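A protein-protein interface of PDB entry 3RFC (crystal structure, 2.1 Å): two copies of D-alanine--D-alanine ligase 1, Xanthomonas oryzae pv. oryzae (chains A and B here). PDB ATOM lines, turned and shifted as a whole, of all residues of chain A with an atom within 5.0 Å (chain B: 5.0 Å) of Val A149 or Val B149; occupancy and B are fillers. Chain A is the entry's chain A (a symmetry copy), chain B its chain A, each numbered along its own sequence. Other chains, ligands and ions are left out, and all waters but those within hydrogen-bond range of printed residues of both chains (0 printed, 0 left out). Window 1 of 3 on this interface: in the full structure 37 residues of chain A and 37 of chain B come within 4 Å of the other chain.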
ATOM      1  N   ASP A 130      12.218 -24.800 -19.388  1.00  0.00           N
ATOM      2  CA  ASP A 130      11.826 -24.126 -18.151  1.00  0.00           C
ATOM      3  C   ASP A 130      11.185 -22.772 -18.424  1.00  0.00           C
ATOM      4  O   ASP A 130      10.918 -22.010 -17.505  1.00  0.00           O
ATOM      5  CB  ASP A 130      12.988 -24.008 -17.136  1.00  0.00           C
ATOM      6  CG  ASP A 130      14.041 -22.989 -17.536  1.00  0.00           C
ATOM      7  OD1 ASP A 130      15.043 -22.839 -16.786  1.00  0.00           O
ATOM      8  OD2 ASP A 130      13.909 -22.290 -18.598  1.00  0.00           O
ATOM      9  N   GLY A 131      10.952 -22.464 -19.693  1.00  0.00           N
ATOM     10  CA  GLY A 131      10.303 -21.211 -20.054  1.00  0.00           C
ATOM     11  C   GLY A 131      11.266 -20.243 -20.668  1.00  0.00           C
ATOM     12  O   GLY A 131      10.833 -19.235 -21.158  1.00  0.00           O
ATOM     13  N   SER A 132      12.594 -20.467 -20.537  1.00  0.00           N
ATOM     14  CA  SER A 132      13.563 -19.486 -20.965  1.00  0.00           C
ATOM     15  C   SER A 132      13.515 -19.409 -22.490  1.00  0.00           C
ATOM     16  O   SER A 132      13.515 -18.355 -23.016  1.00  0.00           O
ATOM     17  CB  SER A 132      15.011 -19.868 -20.573  1.00  0.00           C
ATOM     18  OG  SER A 132      15.138 -20.155 -19.184  1.00  0.00           O
ATOM     19  N   GLN A 134      11.095 -20.375 -24.447  1.00  0.00           N
ATOM     20  CA  GLN A 134       9.801 -19.830 -24.785  1.00  0.00           C
ATOM     21  C   GLN A 134       9.829 -18.297 -24.668  1.00  0.00           C
ATOM     22  O   GLN A 134       9.233 -17.595 -25.512  1.00  0.00           O
ATOM     23  CB  GLN A 134       8.654 -20.451 -23.898  1.00  0.00           C
ATOM     24  CG  GLN A 134       8.435 -21.985 -23.992  1.00  0.00           C
ATOM     25  CD  GLN A 134       9.609 -22.859 -23.512  1.00  0.00           C
ATOM     26  OE1 GLN A 134      10.394 -22.445 -22.658  1.00  0.00           O
ATOM     27  NE2 GLN A 134       9.726 -24.077 -24.057  1.00  0.00           N
ATOM     28  N   GLY A 135      10.557 -17.760 -23.675  1.00  0.00           N
ATOM     29  CA  GLY A 135      10.587 -16.311 -23.560  1.00  0.00           C
ATOM     30  C   GLY A 135      11.389 -15.622 -24.652  1.00  0.00           C
ATOM     31  O   GLY A 135      11.069 -14.500 -25.048  1.00  0.00           O
ATOM     32  N   ARG A 138       8.850 -15.604 -27.659  1.00  0.00           N
ATOM     33  CA  ARG A 138       8.048 -14.383 -27.443  1.00  0.00           C
ATOM     34  C   ARG A 138       8.725 -13.078 -27.749  1.00  0.00           C
ATOM     35  O   ARG A 138       8.105 -12.130 -28.277  1.00  0.00           O
ATOM     36  CB  ARG A 138       7.540 -14.315 -25.993  1.00  0.00           C
ATOM     37  CG  ARG A 138       6.472 -15.361 -25.791  1.00  0.00           C
ATOM     38  CD  ARG A 138       5.935 -15.408 -24.405  1.00  0.00           C
ATOM     39  NE  ARG A 138       5.434 -14.115 -23.892  1.00  0.00           N
ATOM     40  CZ  ARG A 138       4.220 -13.606 -24.063  1.00  0.00           C
ATOM     41  NH1 ARG A 138       3.298 -14.228 -24.772  1.00  0.00           N
ATOM     42  NH2 ARG A 138       3.933 -12.441 -23.510  1.00  0.00           N
ATOM     43  N   SER A 147       3.761 -25.149 -24.185  1.00  0.00           N
ATOM     44  CA  SER A 147       3.380 -24.160 -23.180  1.00  0.00           C
ATOM     45  C   SER A 147       4.178 -22.869 -23.273  1.00  0.00           C
ATOM     46  O   SER A 147       5.312 -22.849 -23.715  1.00  0.00           O
ATOM     47  CB  SER A 147       3.399 -24.723 -21.753  1.00  0.00           C
ATOM     48  OG  SER A 147       2.624 -25.893 -21.641  1.00  0.00           O
ATOM     49  N   GLY A 148       3.530 -21.777 -22.932  1.00  0.00           N
ATOM     50  CA  GLY A 148       4.183 -20.468 -22.912  1.00  0.00           C
ATOM     51  C   GLY A 148       5.116 -20.385 -21.677  1.00  0.00           C
ATOM     52  O   GLY A 148       5.472 -21.394 -21.108  1.00  0.00           O
ATOM     53  N   VAL A 149       5.478 -19.180 -21.279  1.00  0.00           N
ATOM     54  CA  VAL A 149       6.512 -18.976 -20.286  1.00  0.00           C
ATOM     55  C   VAL A 149       6.117 -19.550 -18.933  1.00  0.00           C
ATOM     56  O   VAL A 149       6.860 -20.351 -18.309  1.00  0.00           O
ATOM     57  CB  VAL A 149       6.845 -17.445 -20.274  1.00  0.00           C
ATOM     58  CG1 VAL A 149       7.950 -17.097 -19.195  1.00  0.00           C
ATOM     59  CG2 VAL A 149       7.445 -17.076 -21.656  1.00  0.00           C
ATOM     60  N   LEU A 150       4.908 -19.183 -18.506  1.00  0.00           N
ATOM     61  CA  LEU A 150       4.399 -19.489 -17.201  1.00  0.00           C
ATOM     62  C   LEU A 150       4.149 -20.961 -17.069  1.00  0.00           C
ATOM     63  O   LEU A 150       4.667 -21.607 -16.123  1.00  0.00           O
ATOM     64  CB  LEU A 150       3.097 -18.656 -16.927  1.00  0.00           C
ATOM     65  CG  LEU A 150       2.300 -18.913 -15.615  1.00  0.00           C
ATOM     66  CD1 LEU A 150       3.151 -18.671 -14.352  1.00  0.00           C
ATOM     67  CD2 LEU A 150       1.091 -18.050 -15.545  1.00  0.00           C
ATOM     68  N   GLY A 151       3.352 -21.541 -17.984  1.00  0.00           N
ATOM     69  CA  GLY A 151       3.049 -22.994 -17.891  1.00  0.00           C
ATOM     70  C   GLY A 151       4.336 -23.852 -17.871  1.00  0.00           C
ATOM     71  O   GLY A 151       4.410 -24.855 -17.169  1.00  0.00           O
ATOM     72  N   SER A 152       5.337 -23.436 -18.642  1.00  0.00           N
ATOM     73  CA  SER A 152       6.607 -24.197 -18.730  1.00  0.00           C
ATOM     74  C   SER A 152       7.409 -24.032 -17.428  1.00  0.00           C
ATOM     75  O   SER A 152       7.840 -25.010 -16.853  1.00  0.00           O
ATOM     76  CB  SER A 152       7.464 -23.726 -19.918  1.00  0.00           C
ATOM     77  OG  SER A 152       6.766 -23.783 -21.166  1.00  0.00           O
ATOM     78  N   ALA A 153       7.549 -22.786 -16.984  1.00  0.00           N
ATOM     79  CA  ALA A 153       8.277 -22.432 -15.741  1.00  0.00           C
ATOM     80  C   ALA A 153       7.646 -23.188 -14.584  1.00  0.00           C
ATOM     81  O   ALA A 153       8.363 -23.833 -13.812  1.00  0.00           O
ATOM     82  CB  ALA A 153       8.221 -20.920 -15.500  1.00  0.00           C
ATOM     83  N   VAL A 154       6.306 -23.112 -14.447  1.00  0.00           N
ATOM     84  CA  VAL A 154       5.629 -23.747 -13.321  1.00  0.00           C
ATOM     85  C   VAL A 154       5.730 -25.313 -13.336  1.00  0.00           C
ATOM     86  O   VAL A 154       5.998 -25.988 -12.305  1.00  0.00           O
ATOM     87  CB  VAL A 154       4.154 -23.288 -13.257  1.00  0.00           C
ATOM     88  CG1 VAL A 154       3.448 -24.083 -12.218  1.00  0.00           C
ATOM     89  CG2 VAL A 154       4.066 -21.820 -12.829  1.00  0.00           C
ATOM     90  N   ASP B 130       7.098 -10.269 -17.620  1.00  0.00           N
ATOM     91  CA  ASP B 130       6.367 -11.516 -17.398  1.00  0.00           C
ATOM     92  C   ASP B 130       7.282 -12.730 -17.482  1.00  0.00           C
ATOM     93  O   ASP B 130       6.822 -13.863 -17.457  1.00  0.00           O
ATOM     94  CB  ASP B 130       5.140 -11.667 -18.328  1.00  0.00           C
ATOM     95  CG  ASP B 130       5.507 -11.961 -19.773  1.00  0.00           C
ATOM     96  OD1 ASP B 130       4.576 -12.076 -20.614  1.00  0.00           O
ATOM     97  OD2 ASP B 130       6.728 -12.105 -20.124  1.00  0.00           O
ATOM     98  N   GLY B 131       8.583 -12.493 -17.599  1.00  0.00           N
ATOM     99  CA  GLY B 131       9.544 -13.588 -17.642  1.00  0.00           C
ATOM    100  C   GLY B 131      10.111 -13.775 -19.016  1.00  0.00           C
ATOM    101  O   GLY B 131      11.031 -14.534 -19.159  1.00  0.00           O
ATOM    102  N   SER B 132       9.491 -13.189 -20.066  1.00  0.00           N
ATOM    103  CA  SER B 132       9.896 -13.468 -21.423  1.00  0.00           C
ATOM    104  C   SER B 132      11.282 -12.862 -21.637  1.00  0.00           C
ATOM    105  O   SER B 132      12.110 -13.493 -22.187  1.00  0.00           O
ATOM    106  CB  SER B 132       8.953 -12.828 -22.471  1.00  0.00           C
ATOM    107  OG  SER B 132       7.588 -13.173 -22.253  1.00  0.00           O
ATOM    108  N   GLN B 134      13.449 -12.024 -19.352  1.00  0.00           N
ATOM    109  CA  GLN B 134      14.353 -12.770 -18.506  1.00  0.00           C
ATOM    110  C   GLN B 134      14.771 -14.074 -19.203  1.00  0.00           C
ATOM    111  O   GLN B 134      15.949 -14.478 -19.116  1.00  0.00           O
ATOM    112  CB  GLN B 134      13.724 -13.054 -17.087  1.00  0.00           C
ATOM    113  CG  GLN B 134      13.346 -11.825 -16.218  1.00  0.00           C
ATOM    114  CD  GLN B 134      12.243 -10.915 -16.790  1.00  0.00           C
ATOM    115  OE1 GLN B 134      11.382 -11.369 -17.544  1.00  0.00           O
ATOM    116  NE2 GLN B 134      12.264  -9.626 -16.424  1.00  0.00           N
ATOM    117  N   GLY B 135      13.849 -14.711 -19.942  1.00  0.00           N
ATOM    118  CA  GLY B 135      14.240 -15.945 -20.604  1.00  0.00           C
ATOM    119  C   GLY B 135      15.183 -15.743 -21.778  1.00  0.00           C
ATOM    120  O   GLY B 135      16.024 -16.600 -22.059  1.00  0.00           O
ATOM    121  N   ARG B 138      18.655 -15.284 -19.985  1.00  0.00           N
ATOM    122  CA  ARG B 138      19.145 -16.664 -19.796  1.00  0.00           C
ATOM    123  C   ARG B 138      19.649 -17.367 -21.023  1.00  0.00           C
ATOM    124  O   ARG B 138      20.642 -18.125 -20.980  1.00  0.00           O
ATOM    125  CB  ARG B 138      18.055 -17.549 -19.169  1.00  0.00           C
ATOM    126  CG  ARG B 138      17.856 -17.149 -17.728  1.00  0.00           C
ATOM    127  CD  ARG B 138      16.793 -17.920 -17.032  1.00  0.00           C
ATOM    128  NE  ARG B 138      16.950 -19.388 -17.098  1.00  0.00           N
ATOM    129  CZ  ARG B 138      17.666 -20.151 -16.282  1.00  0.00           C
ATOM    130  NH1 ARG B 138      18.371 -19.639 -15.293  1.00  0.00           N
ATOM    131  NH2 ARG B 138      17.675 -21.458 -16.474  1.00  0.00           N
ATOM    132  N   SER B 147      13.923 -10.753 -10.703  1.00  0.00           N
ATOM    133  CA  SER B 147      13.503 -12.151 -10.667  1.00  0.00           C
ATOM    134  C   SER B 147      13.775 -12.896 -11.964  1.00  0.00           C
ATOM    135  O   SER B 147      13.806 -12.320 -13.037  1.00  0.00           O
ATOM    136  CB  SER B 147      12.044 -12.323 -10.224  1.00  0.00           C
ATOM    137  OG  SER B 147      11.789 -11.678  -8.999  1.00  0.00           O
ATOM    138  N   GLY B 148      14.061 -14.172 -11.835  1.00  0.00           N
ATOM    139  CA  GLY B 148      14.288 -15.033 -12.996  1.00  0.00           C
ATOM    140  C   GLY B 148      12.927 -15.333 -13.678  1.00  0.00           C
ATOM    141  O   GLY B 148      11.962 -14.636 -13.455  1.00  0.00           O
ATOM    142  N   VAL B 149      12.879 -16.380 -14.480  1.00  0.00           N
ATOM    143  CA  VAL B 149      11.741 -16.636 -15.341  1.00  0.00           C
ATOM    144  C   VAL B 149      10.477 -16.909 -14.539  1.00  0.00           C
ATOM    145  O   VAL B 149       9.411 -16.273 -14.742  1.00  0.00           O
ATOM    146  CB  VAL B 149      12.154 -17.786 -16.321  1.00  0.00           C
ATOM    147  CG1 VAL B 149      10.968 -18.175 -17.295  1.00  0.00           C
ATOM    148  CG2 VAL B 149      13.306 -17.260 -17.216  1.00  0.00           C
ATOM    149  N   LEU B 150      10.616 -17.821 -13.576  1.00  0.00           N
ATOM    150  CA  LEU B 150       9.524 -18.333 -12.801  1.00  0.00           C
ATOM    151  C   LEU B 150       8.978 -17.268 -11.899  1.00  0.00           C
ATOM    152  O   LEU B 150       7.755 -16.982 -11.928  1.00  0.00           O
ATOM    153  CB  LEU B 150       9.989 -19.593 -11.988  1.00  0.00           C
ATOM    154  CG  LEU B 150       8.999 -20.247 -10.981  1.00  0.00           C
ATOM    155  CD1 LEU B 150       7.697 -20.720 -11.658  1.00  0.00           C
ATOM    156  CD2 LEU B 150       9.625 -21.409 -10.294  1.00  0.00           C
ATOM    157  N   GLY B 151       9.840 -16.655 -11.068  1.00  0.00           N
ATOM    158  CA  GLY B 151       9.352 -15.605 -10.135  1.00  0.00           C
ATOM    159  C   GLY B 151       8.623 -14.462 -10.880  1.00  0.00           C
ATOM    160  O   GLY B 151       7.633 -13.926 -10.392  1.00  0.00           O
ATOM    161  N   SER B 152       9.124 -14.110 -12.061  1.00  0.00           N
ATOM    162  CA  SER B 152       8.531 -13.005 -12.850  1.00  0.00           C
ATOM    163  C   SER B 152       7.183 -13.448 -13.443  1.00  0.00           C
ATOM    164  O   SER B 152       6.198 -12.753 -13.299  1.00  0.00           O
ATOM    165  CB  SER B 152       9.466 -12.561 -13.989  1.00  0.00           C
ATOM    166  OG  SER B 152      10.769 -12.194 -13.529  1.00  0.00           O
ATOM    167  N   ALA B 153       7.178 -14.626 -14.062  1.00  0.00           N
ATOM    168  CA  ALA B 153       5.971 -15.224 -14.684  1.00  0.00           C
ATOM    169  C   ALA B 153       4.892 -15.341 -13.621  1.00  0.00           C
ATOM    170  O   ALA B 153       3.758 -14.909 -13.850  1.00  0.00           O
ATOM    171  CB  ALA B 153       6.300 -16.597 -15.279  1.00  0.00           C
ATOM    172  N   VAL B 154       5.229 -15.929 -12.453  1.00  0.00           N
ATOM    173  CA  VAL B 154       4.234 -16.147 -11.409  1.00  0.00           C
ATOM    174  C   VAL B 154       3.672 -14.816 -10.795  1.00  0.00           C
ATOM    175  O   VAL B 154       2.444 -14.632 -10.579  1.00  0.00           O
ATOM    176  CB  VAL B 154       4.810 -17.064 -10.306  1.00  0.00           C
ATOM    177  CG1 VAL B 154       3.846 -17.122  -9.176  1.00  0.00           C
ATOM    178  CG2 VAL B 154       4.970 -18.496 -10.827  1.00  0.00           C
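OG of Ser B132 is in hydrogen-bond range of OD2 of Asp B130 (2.5 Å). The backbone carbonyl oxygen (O) of Asp B130 sits close to the backbone NH (N) of Ala B153, 3.5 Å away. N of Gly B131 lies close to OE1 of Gln B134 (3.0 Å). The side-chain hydroxyl of Ser A132 sits at hydrogen-bond distance from the side-chain carboxylate of Asp A130. N of Ala A153 lies close to O of Asp A130, at 3.5 Å. N of Gly A131 sits close to OE1 of Gln A134 (3.0 Å).
Printed residues of chain A within 4 Å of Val B149: Asp A130 (3.8 Å), Gly A131 (3.97 Å), Ser A132 (3.95 Å) and Val A149 (3.7 Å). Of the printed residues of chain A, Arg B138 touches Asp A130 (3.0 Å) and Ser A132 (2.9 Å). Of the printed residues of chain A, Gly B135 touches Ser A132. Ser A152 touches none of the printed residues of chain B. The nearest residue of chain B that does not touch Val A149 is Ala B153 (4.3 Å). The nearest residue of chain A that does not touch Val B149 is Ala A153 (4.3 Å).
Asp A130 touches Val B149, and with the chains exchanged Val A149 touches Asp B130. Ser A132 touches Val B149, and with the chains exchanged Val A149 touches Ser B132. Leu A150 touches Ala B153, and with the chains exchanged Ala A153 touches Leu B150. Val B154 touches its own counterpart, Val A154. Of the 18 pairs that touch across the chains among the printed residues, 18 have their exchanged pair printed and touching as well.
Hydrophobic or aromatic side chains of chain A that line the printed part of chain B: Val A149, Leu A150, Ala A153 and Val A154. Of the 14 printed residues of chain B, 9 touch a printed residue of chain A. Among the printed residues, Asp or Glu carboxylates within 4 Å of a Lys or Arg side-chain nitrogen of the other chain: Asp A130 with Arg B138 and Arg A138 with Asp B130.
The guanidinium group (NH2) of Arg A138 is in salt-bridge range of the side-chain carboxylate (OD1) of Asp B130, at 3.0 Å. NE of Arg A138 is in hydrogen-bond range of OG of Ser B132 (2.9 Å). The guanidinium group of Arg B138 lies within salt-bridge range of the side-chain carboxylate of Asp A130, at 3.0 Å. NE of Arg B138 lies within hydrogen-bond range of OG of Ser A132 (2.9 Å). O of Gly B135 lies close to O of Ser A132 (3.2 Å). O of Gly A135 lies close to O of Ser B132 (3.2 Å).
CG1 of Val B149 touches C of Gly A131, at 3.97 Å. Val B149 touches Ser A132. Val A149 touches Asp B130 (CG1 to O, 3.8 Å). Val A149 touches Gly B131. Ser B132 touches Val A149. Val B149 touches Val A149 (CG1 to CG1, 3.7 Å). Ala B153 touches Leu A150 (C to CD1, 3.8 Å). Leu B150 touches Ala A153. Val A154 touches Leu B150. Val A154 touches Val B154 (CG2 to CG2, 3.98 Å).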
